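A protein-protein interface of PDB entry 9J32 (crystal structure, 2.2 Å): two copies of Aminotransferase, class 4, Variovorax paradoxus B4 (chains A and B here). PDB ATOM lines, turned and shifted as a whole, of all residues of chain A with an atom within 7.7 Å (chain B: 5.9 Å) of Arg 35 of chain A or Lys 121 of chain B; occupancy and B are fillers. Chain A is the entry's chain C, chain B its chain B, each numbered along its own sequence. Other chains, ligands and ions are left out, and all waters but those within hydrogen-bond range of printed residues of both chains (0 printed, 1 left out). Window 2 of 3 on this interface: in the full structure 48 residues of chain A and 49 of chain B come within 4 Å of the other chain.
O of Ala 38 of chain A sits at hydrogen-bond distance from N of Val 42 of chain B.
The side-chain carboxylate (OE1) of Glu 141 of chain A sits at hydrogen-bond distance from the side-chain hydroxyl (OG1) of Thr 122 of chain B (2.7 Å).
The guanidinium group (NH2) of Arg 35 of chain A sits at hydrogen-bond distance from the backbone carbonyl oxygen (O) of Lys 121 of chain B (3.2 Å).
Arg 35 of chain A touches just these residues of chain B: Phe 43 and Lys 121.
Lys 121 of chain B touches one residue of chain A.
Printed residues of chain B within 4 Å of Val 139 of chain A: Phe 43 (3.8 Å).
Of the printed residues of chain B, Glu 141 of chain A touches Thr 122 and Pro 123.
Of the printed residues of chain A, Val 42 of chain B touches Ala 38 (3.0 Å) and Val 39 (3.8 Å).
The nearest residue of chain B that does not touch Arg 35 of chain A is Lys 120 of chain B (4.6 Å).
The nearest printed residue of chain A that does not touch Ser 41 of chain B is Val 39 of chain A (4.2 Å).
Among the printed residues, pairs that only touch across the chains: Arg 35 of chain A with Phe 43 of chain B (3.4 Å), Ala 38 of chain A with Ser 41 of chain B (3.5 Å), Val 39 of chain A with Val 42 of chain B (3.8 Å), Val 139 of chain A with Phe 43 of chain B (3.8 Å) and Glu 141 of chain A with Pro 123 of chain B (3.6 Å).
No position is printed for both chains.
Of the 8 pairs that touch across the chains among the printed residues, none has its exchanged pair printed and touching as well.
Of the 10 printed residues of chain B, 6 touch a printed residue of chain A.
Printed residues of chain B that touch a printed residue of chain A: Ser 41, Val 42, Phe 43, Lys 121, Thr 122 and Pro 123.
Hydrophobic or aromatic side chains of chain B that line the printed part of chain A: Val 42, Phe 43 and Pro 123.
Among the printed residues, 8 pairs touch across the chains.
Among the printed residues, no Asp or Glu carboxylate lies within 4 Å of a Lys or Arg side-chain nitrogen of the other chain.
The guanidinium group (NH1) of Arg 35 of chain A lies within salt-bridge range of the side-chain carboxylate (OE2) of Glu 141 of chain A, at 3.1 Å.
N of Lys 120 of chain B lies within hydrogen-bond range of O of Phe 43 of chain B (3.1 Å).
The backbone NH (N) of Arg 35 of chain A is in hydrogen-bond range of the backbone carbonyl oxygen (O) of Val 24 of chain A, at 3.2 Å.
The side-chain hydroxyl (OG) of Ser 41 of chain B lies within hydrogen-bond range of the backbone NH (N) of Phe 43 of chain B (3.0 Å).
The backbone carbonyl oxygen (O) of Asn 21 of chain A lies within hydrogen-bond range of the guanidinium group (NE) of Arg 35 of chain A, at 3.1 Å.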
ATOM      1  N   ASP A  18      20.944  -5.152   7.259  1.00  0.00           N
ATOM      2  CA  ASP A  18      21.744  -3.955   7.069  1.00  0.00           C
ATOM      3  C   ASP A  18      20.874  -2.863   6.449  1.00  0.00           C
ATOM      4  O   ASP A  18      20.378  -3.020   5.334  1.00  0.00           O
ATOM      5  CB  ASP A  18      22.982  -4.269   6.254  1.00  0.00           C
ATOM      6  CG  ASP A  18      23.966  -3.147   5.959  1.00  0.00           C
ATOM      7  OD1 ASP A  18      23.670  -1.995   6.234  1.00  0.00           O
ATOM      8  OD2 ASP A  18      25.061  -3.455   5.492  1.00  0.00           O
ATOM      9  N   ARG A  20      21.580  -0.142   5.065  1.00  0.00           N
ATOM     10  CA  ARG A  20      22.036   0.403   3.796  1.00  0.00           C
ATOM     11  C   ARG A  20      21.289  -0.230   2.618  1.00  0.00           C
ATOM     12  O   ARG A  20      21.122   0.406   1.568  1.00  0.00           O
ATOM     13  CB  ARG A  20      23.557   0.212   3.701  1.00  0.00           C
ATOM     14  CG  ARG A  20      24.300   1.055   4.734  1.00  0.00           C
ATOM     15  CD  ARG A  20      25.791   0.914   4.565  1.00  0.00           C
ATOM     16  NE  ARG A  20      26.251  -0.444   4.869  1.00  0.00           N
ATOM     17  CZ  ARG A  20      27.493  -0.874   4.680  1.00  0.00           C
ATOM     18  NH1 ARG A  20      28.437  -0.009   4.372  1.00  0.00           N
ATOM     19  NH2 ARG A  20      27.800  -2.141   4.837  1.00  0.00           N
ATOM     20  N   ASN A  21      20.795  -1.462   2.801  1.00  0.00           N
ATOM     21  CA  ASN A  21      19.984  -2.118   1.780  1.00  0.00           C
ATOM     22  C   ASN A  21      18.795  -1.268   1.337  1.00  0.00           C
ATOM     23  O   ASN A  21      18.472  -1.325   0.143  1.00  0.00           O
ATOM     24  CB  ASN A  21      19.646  -3.551   2.188  1.00  0.00           C
ATOM     25  CG  ASN A  21      20.886  -4.409   2.141  1.00  0.00           C
ATOM     26  OD1 ASN A  21      21.895  -3.987   1.577  1.00  0.00           O
ATOM     27  ND2 ASN A  21      20.827  -5.629   2.650  1.00  0.00           N
ATOM     28  N   ASP A  22      18.242  -0.428   2.239  1.00  0.00           N
ATOM     29  CA  ASP A  22      17.022   0.311   1.946  1.00  0.00           C
ATOM     30  C   ASP A  22      17.207   1.433   0.924  1.00  0.00           C
ATOM     31  O   ASP A  22      16.198   1.857   0.358  1.00  0.00           O
ATOM     32  CB  ASP A  22      16.346   0.791   3.215  1.00  0.00           C
ATOM     33  CG  ASP A  22      15.967  -0.306   4.202  1.00  0.00           C
ATOM     34  OD1 ASP A  22      15.872  -1.470   3.800  1.00  0.00           O
ATOM     35  OD2 ASP A  22      15.772   0.007   5.372  1.00  0.00           O
ATOM     36  N   ALA A  23      18.453   1.884   0.677  1.00  0.00           N
ATOM     37  CA  ALA A  23      18.733   3.027  -0.188  1.00  0.00           C
ATOM     38  C   ALA A  23      19.665   2.684  -1.354  1.00  0.00           C
ATOM     39  O   ALA A  23      20.162   3.604  -2.005  1.00  0.00           O
ATOM     40  CB  ALA A  23      19.305   4.158   0.662  1.00  0.00           C
ATOM     41  N   VAL A  24      19.923   1.391  -1.634  1.00  0.00           N
ATOM     42  CA  VAL A  24      20.761   0.992  -2.773  1.00  0.00           C
ATOM     43  C   VAL A  24      20.120   1.499  -4.077  1.00  0.00           C
ATOM     44  O   VAL A  24      18.875   1.611  -4.166  1.00  0.00           O
ATOM     45  CB  VAL A  24      21.009  -0.537  -2.857  1.00  0.00           C
ATOM     46  CG1 VAL A  24      21.798  -1.059  -1.662  1.00  0.00           C
ATOM     47  CG2 VAL A  24      19.723  -1.328  -3.051  1.00  0.00           C
ATOM     48  N   LEU A  25      20.973   1.869  -5.048  1.00  0.00           N
ATOM     49  CA  LEU A  25      20.532   2.164  -6.407  1.00  0.00           C
ATOM     50  C   LEU A  25      20.584   0.870  -7.222  1.00  0.00           C
ATOM     51  O   LEU A  25      21.520   0.079  -7.086  1.00  0.00           O
ATOM     52  CB  LEU A  25      21.364   3.251  -7.090  1.00  0.00           C
ATOM     53  CG  LEU A  25      21.246   4.686  -6.549  1.00  0.00           C
ATOM     54  CD1 LEU A  25      22.384   5.514  -7.156  1.00  0.00           C
ATOM     55  CD2 LEU A  25      19.914   5.401  -6.796  1.00  0.00           C
ATOM     56  N   VAL A  26      19.581   0.683  -8.094  1.00  0.00           N
ATOM     57  CA  VAL A  26      19.432  -0.517  -8.913  1.00  0.00           C
ATOM     58  C   VAL A  26      19.705  -0.111 -10.356  1.00  0.00           C
ATOM     59  O   VAL A  26      19.289   0.963 -10.783  1.00  0.00           O
ATOM     60  CB  VAL A  26      17.998  -1.082  -8.758  1.00  0.00           C
ATOM     61  CG1 VAL A  26      17.758  -2.298  -9.630  1.00  0.00           C
ATOM     62  CG2 VAL A  26      17.666  -1.384  -7.301  1.00  0.00           C
ATOM     63  N   PHE A  32      20.380   4.404 -13.066  1.00  0.00           N
ATOM     64  CA  PHE A  32      20.533   3.960 -11.687  1.00  0.00           C
ATOM     65  C   PHE A  32      19.409   4.553 -10.855  1.00  0.00           C
ATOM     66  O   PHE A  32      19.339   5.776 -10.709  1.00  0.00           O
ATOM     67  CB  PHE A  32      21.890   4.317 -11.079  1.00  0.00           C
ATOM     68  CG  PHE A  32      23.000   3.418 -11.585  1.00  0.00           C
ATOM     69  CD1 PHE A  32      23.197   2.177 -11.010  1.00  0.00           C
ATOM     70  CD2 PHE A  32      23.797   3.783 -12.651  1.00  0.00           C
ATOM     71  CE1 PHE A  32      24.169   1.306 -11.499  1.00  0.00           C
ATOM     72  CE2 PHE A  32      24.812   2.950 -13.108  1.00  0.00           C
ATOM     73  CZ  PHE A  32      24.996   1.710 -12.527  1.00  0.00           C
ATOM     74  N   VAL A  33      18.592   3.692 -10.250  1.00  0.00           N
ATOM     75  CA  VAL A  33      17.282   4.076  -9.731  1.00  0.00           C
ATOM     76  C   VAL A  33      17.173   3.661  -8.259  1.00  0.00           C
ATOM     77  O   VAL A  33      17.641   2.599  -7.874  1.00  0.00           O
ATOM     78  CB  VAL A  33      16.259   3.398 -10.673  1.00  0.00           C
ATOM     79  CG1 VAL A  33      14.924   3.105 -10.026  1.00  0.00           C
ATOM     80  CG2 VAL A  33      16.068   4.239 -11.935  1.00  0.00           C
ATOM     81  N   PRO A  34      16.574   4.487  -7.368  1.00  0.00           N
ATOM     82  CA  PRO A  34      16.273   4.055  -6.002  1.00  0.00           C
ATOM     83  C   PRO A  34      15.482   2.760  -5.954  1.00  0.00           C
ATOM     84  O   PRO A  34      14.547   2.602  -6.743  1.00  0.00           O
ATOM     85  CB  PRO A  34      15.422   5.170  -5.454  1.00  0.00           C
ATOM     86  CG  PRO A  34      15.987   6.361  -6.207  1.00  0.00           C
ATOM     87  CD  PRO A  34      16.240   5.901  -7.589  1.00  0.00           C
ATOM     88  N   ARG A  35      15.807   1.882  -4.997  1.00  0.00           N
ATOM     89  CA  ARG A  35      15.219   0.539  -4.962  1.00  0.00           C
ATOM     90  C   ARG A  35      13.673   0.556  -4.873  1.00  0.00           C
ATOM     91  O   ARG A  35      13.019  -0.352  -5.427  1.00  0.00           O
ATOM     92  CB  ARG A  35      15.914  -0.307  -3.881  1.00  0.00           C
ATOM     93  CG  ARG A  35      15.682   0.127  -2.436  1.00  0.00           C
ATOM     94  CD  ARG A  35      14.966  -0.920  -1.595  1.00  0.00           C
ATOM     95  NE  ARG A  35      15.843  -2.072  -1.398  1.00  0.00           N
ATOM     96  CZ  ARG A  35      15.491  -3.312  -1.172  1.00  0.00           C
ATOM     97  NH1 ARG A  35      16.284  -4.056  -0.423  1.00  0.00           N
ATOM     98  NH2 ARG A  35      14.351  -3.814  -1.615  1.00  0.00           N
ATOM     99  N   HIS A  36      13.111   1.599  -4.213  1.00  0.00           N
ATOM    100  CA  HIS A  36      11.670   1.809  -4.096  1.00  0.00           C
ATOM    101  C   HIS A  36      11.058   2.096  -5.469  1.00  0.00           C
ATOM    102  O   HIS A  36       9.841   1.964  -5.626  1.00  0.00           O
ATOM    103  CB  HIS A  36      11.337   2.993  -3.157  1.00  0.00           C
ATOM    104  N   GLN A  37      11.880   2.553  -6.444  1.00  0.00           N
ATOM    105  CA  GLN A  37      11.394   2.981  -7.745  1.00  0.00           C
ATOM    106  C   GLN A  37      11.996   2.150  -8.866  1.00  0.00           C
ATOM    107  O   GLN A  37      11.821   2.524 -10.017  1.00  0.00           O
ATOM    108  CB  GLN A  37      11.719   4.469  -7.888  1.00  0.00           C
ATOM    109  CG  GLN A  37      11.205   5.342  -6.747  1.00  0.00           C
ATOM    110  CD  GLN A  37      11.925   6.663  -6.650  1.00  0.00           C
ATOM    111  OE1 GLN A  37      12.721   7.055  -7.519  1.00  0.00           O
ATOM    112  NE2 GLN A  37      11.674   7.334  -5.540  1.00  0.00           N
ATOM    113  N   ALA A  38      12.654   1.010  -8.550  1.00  0.00           N
ATOM    114  CA  ALA A  38      13.184   0.138  -9.582  1.00  0.00           C
ATOM    115  C   ALA A  38      12.040  -0.744 -10.083  1.00  0.00           C
ATOM    116  O   ALA A  38      11.516  -1.527  -9.309  1.00  0.00           O
ATOM    117  CB  ALA A  38      14.366  -0.674  -9.080  1.00  0.00           C
ATOM    118  N   VAL A  39      11.718  -0.609 -11.377  1.00  0.00           N
ATOM    119  CA  VAL A  39      10.511  -1.098 -12.009  1.00  0.00           C
ATOM    120  C   VAL A  39      10.849  -1.579 -13.434  1.00  0.00           C
ATOM    121  O   VAL A  39      11.795  -1.087 -14.099  1.00  0.00           O
ATOM    122  CB  VAL A  39       9.349  -0.092 -12.037  1.00  0.00           C
ATOM    123  CG1 VAL A  39       8.744   0.163 -10.650  1.00  0.00           C
ATOM    124  CG2 VAL A  39       9.730   1.232 -12.673  1.00  0.00           C
ATOM    125  N   VAL A 139      20.546  -5.799  -9.203  1.00  0.00           N
ATOM    126  CA  VAL A 139      20.341  -5.479  -7.799  1.00  0.00           C
ATOM    127  C   VAL A 139      21.588  -5.942  -7.043  1.00  0.00           C
ATOM    128  O   VAL A 139      21.925  -7.139  -7.030  1.00  0.00           O
ATOM    129  CB  VAL A 139      19.078  -6.161  -7.223  1.00  0.00           C
ATOM    130  CG1 VAL A 139      18.852  -5.735  -5.766  1.00  0.00           C
ATOM    131  CG2 VAL A 139      17.813  -5.914  -8.052  1.00  0.00           C
ATOM    132  N   ALA A 140      22.271  -4.992  -6.433  1.00  0.00           N
ATOM    133  CA  ALA A 140      23.358  -5.226  -5.520  1.00  0.00           C
ATOM    134  C   ALA A 140      22.863  -4.899  -4.120  1.00  0.00           C
ATOM    135  O   ALA A 140      22.236  -3.834  -3.938  1.00  0.00           O
ATOM    136  CB  ALA A 140      24.531  -4.380  -5.921  1.00  0.00           C
ATOM    137  N   GLU A 141      23.141  -5.824  -3.173  1.00  0.00           N
ATOM    138  CA  GLU A 141      22.835  -5.644  -1.759  1.00  0.00           C
ATOM    139  C   GLU A 141      24.022  -6.036  -0.876  1.00  0.00           C
ATOM    140  O   GLU A 141      24.880  -6.813  -1.318  1.00  0.00           O
ATOM    141  CB  GLU A 141      21.651  -6.542  -1.436  1.00  0.00           C
ATOM    142  CG  GLU A 141      20.461  -6.294  -2.356  1.00  0.00           C
ATOM    143  CD  GLU A 141      19.135  -6.709  -1.763  1.00  0.00           C
ATOM    144  OE1 GLU A 141      18.620  -7.708  -2.245  1.00  0.00           O
ATOM    145  OE2 GLU A 141      18.628  -6.054  -0.822  1.00  0.00           O
ATOM    146  N   SER B  41       7.440  -3.678  -9.527  1.00  0.00           N
ATOM    147  CA  SER B  41       8.731  -3.614  -8.857  1.00  0.00           C
ATOM    148  C   SER B  41       9.635  -4.747  -9.345  1.00  0.00           C
ATOM    149  O   SER B  41       9.155  -5.864  -9.592  1.00  0.00           O
ATOM    150  CB  SER B  41       8.569  -3.684  -7.357  1.00  0.00           C
ATOM    151  OG  SER B  41       9.842  -3.826  -6.729  1.00  0.00           O
ATOM    152  N   VAL B  42      10.949  -4.472  -9.426  1.00  0.00           N
ATOM    153  CA  VAL B  42      11.907  -5.514  -9.742  1.00  0.00           C
ATOM    154  C   VAL B  42      12.081  -6.503  -8.570  1.00  0.00           C
ATOM    155  O   VAL B  42      12.677  -7.593  -8.766  1.00  0.00           O
ATOM    156  CB  VAL B  42      13.256  -4.970 -10.243  1.00  0.00           C
ATOM    157  CG1 VAL B  42      13.096  -4.116 -11.490  1.00  0.00           C
ATOM    158  CG2 VAL B  42      14.016  -4.228  -9.180  1.00  0.00           C
ATOM    159  N   PHE B  43      11.507  -6.186  -7.385  1.00  0.00           N
ATOM    160  CA  PHE B  43      11.404  -7.141  -6.276  1.00  0.00           C
ATOM    161  C   PHE B  43      10.156  -8.053  -6.321  1.00  0.00           C
ATOM    162  O   PHE B  43       9.950  -8.874  -5.420  1.00  0.00           O
ATOM    163  CB  PHE B  43      11.488  -6.302  -5.000  1.00  0.00           C
ATOM    164  CG  PHE B  43      12.864  -5.662  -4.886  1.00  0.00           C
ATOM    165  CD1 PHE B  43      13.948  -6.405  -4.442  1.00  0.00           C
ATOM    166  CD2 PHE B  43      13.057  -4.341  -5.274  1.00  0.00           C
ATOM    167  CE1 PHE B  43      15.210  -5.872  -4.428  1.00  0.00           C
ATOM    168  CE2 PHE B  43      14.315  -3.764  -5.191  1.00  0.00           C
ATOM    169  CZ  PHE B  43      15.397  -4.536  -4.766  1.00  0.00           C
ATOM    170  N   VAL B 119       5.850  -8.353  -3.613  1.00  0.00           N
ATOM    171  CA  VAL B 119       7.174  -7.790  -3.479  1.00  0.00           C
ATOM    172  C   VAL B 119       7.858  -8.444  -2.274  1.00  0.00           C
ATOM    173  O   VAL B 119       7.208  -8.715  -1.253  1.00  0.00           O
ATOM    174  CB  VAL B 119       7.002  -6.260  -3.291  1.00  0.00           C
ATOM    175  CG1 VAL B 119       8.328  -5.539  -3.062  1.00  0.00           C
ATOM    176  CG2 VAL B 119       6.227  -5.624  -4.445  1.00  0.00           C
ATOM    177  N   LYS B 120       9.179  -8.680  -2.381  1.00  0.00           N
ATOM    178  CA  LYS B 120       9.979  -9.251  -1.298  1.00  0.00           C
ATOM    179  C   LYS B 120      11.069  -8.266  -0.893  1.00  0.00           C
ATOM    180  O   LYS B 120      11.473  -7.452  -1.715  1.00  0.00           O
ATOM    181  CB  LYS B 120      10.619 -10.582  -1.712  1.00  0.00           C
ATOM    182  CG  LYS B 120       9.662 -11.571  -2.370  1.00  0.00           C
ATOM    183  CD  LYS B 120       9.907 -13.047  -2.070  1.00  0.00           C
ATOM    184  CE  LYS B 120       9.398 -14.032  -3.104  1.00  0.00           C
ATOM    185  NZ  LYS B 120      10.077 -14.026  -4.411  1.00  0.00           N
ATOM    186  N   LYS B 121      11.516  -8.343   0.379  1.00  0.00           N
ATOM    187  CA  LYS B 121      12.596  -7.515   0.912  1.00  0.00           C
ATOM    188  C   LYS B 121      13.825  -7.740   0.042  1.00  0.00           C
ATOM    189  O   LYS B 121      14.483  -6.786  -0.345  1.00  0.00           O
ATOM    190  CB  LYS B 121      13.002  -7.758   2.379  1.00  0.00           C
ATOM    191  N   THR B 122      14.068  -9.013  -0.303  1.00  0.00           N
ATOM    192  CA  THR B 122      15.177  -9.429  -1.136  1.00  0.00           C
ATOM    193  C   THR B 122      14.692 -10.533  -2.081  1.00  0.00           C
ATOM    194  O   THR B 122      13.850 -11.346  -1.696  1.00  0.00           O
ATOM    195  CB  THR B 122      16.315  -9.881  -0.218  1.00  0.00           C
ATOM    196  OG1 THR B 122      17.481  -9.809  -1.026  1.00  0.00           O
ATOM    197  CG2 THR B 122      16.237 -11.308   0.310  1.00  0.00           C
ATOM    198  N   PRO B 123      15.215 -10.630  -3.328  1.00  0.00           N
ATOM    199  CA  PRO B 123      14.853 -11.737  -4.204  1.00  0.00           C
ATOM    200  C   PRO B 123      15.309 -13.082  -3.649  1.00  0.00           C
ATOM    201  O   PRO B 123      16.479 -13.274  -3.371  1.00  0.00           O
ATOM    202  CB  PRO B 123      15.477 -11.374  -5.539  1.00  0.00           C
ATOM    203  CG  PRO B 123      16.609 -10.453  -5.166  1.00  0.00           C
ATOM    204  CD  PRO B 123      16.152  -9.691  -3.967  1.00  0.00           C
ATOM    205  N   PHE B 129       8.190 -14.507   2.771  1.00  0.00           N
ATOM    206  CA  PHE B 129       8.914 -13.292   3.127  1.00  0.00           C
ATOM    207  C   PHE B 129       8.329 -12.082   2.355  1.00  0.00           C
ATOM    208  O   PHE B 129       9.082 -11.210   1.943  1.00  0.00           O
ATOM    209  CB  PHE B 129      10.401 -13.703   2.986  1.00  0.00           C
ATOM    210  N   ILE B 131       6.034  -8.605   1.582  1.00  0.00           N
ATOM    211  CA  ILE B 131       5.563  -7.377   2.232  1.00  0.00           C
ATOM    212  C   ILE B 131       4.354  -6.909   1.424  1.00  0.00           C
ATOM    213  O   ILE B 131       4.442  -6.810   0.210  1.00  0.00           O
ATOM    214  CB  ILE B 131       6.636  -6.276   2.455  1.00  0.00           C
ATOM    215  CG1 ILE B 131       6.335  -4.895   1.800  1.00  0.00           C
ATOM    216  CG2 ILE B 131       8.048  -6.768   2.129  1.00  0.00           C
ATOM    217  CD1 ILE B 131       7.500  -3.928   1.887  1.00  0.00           C
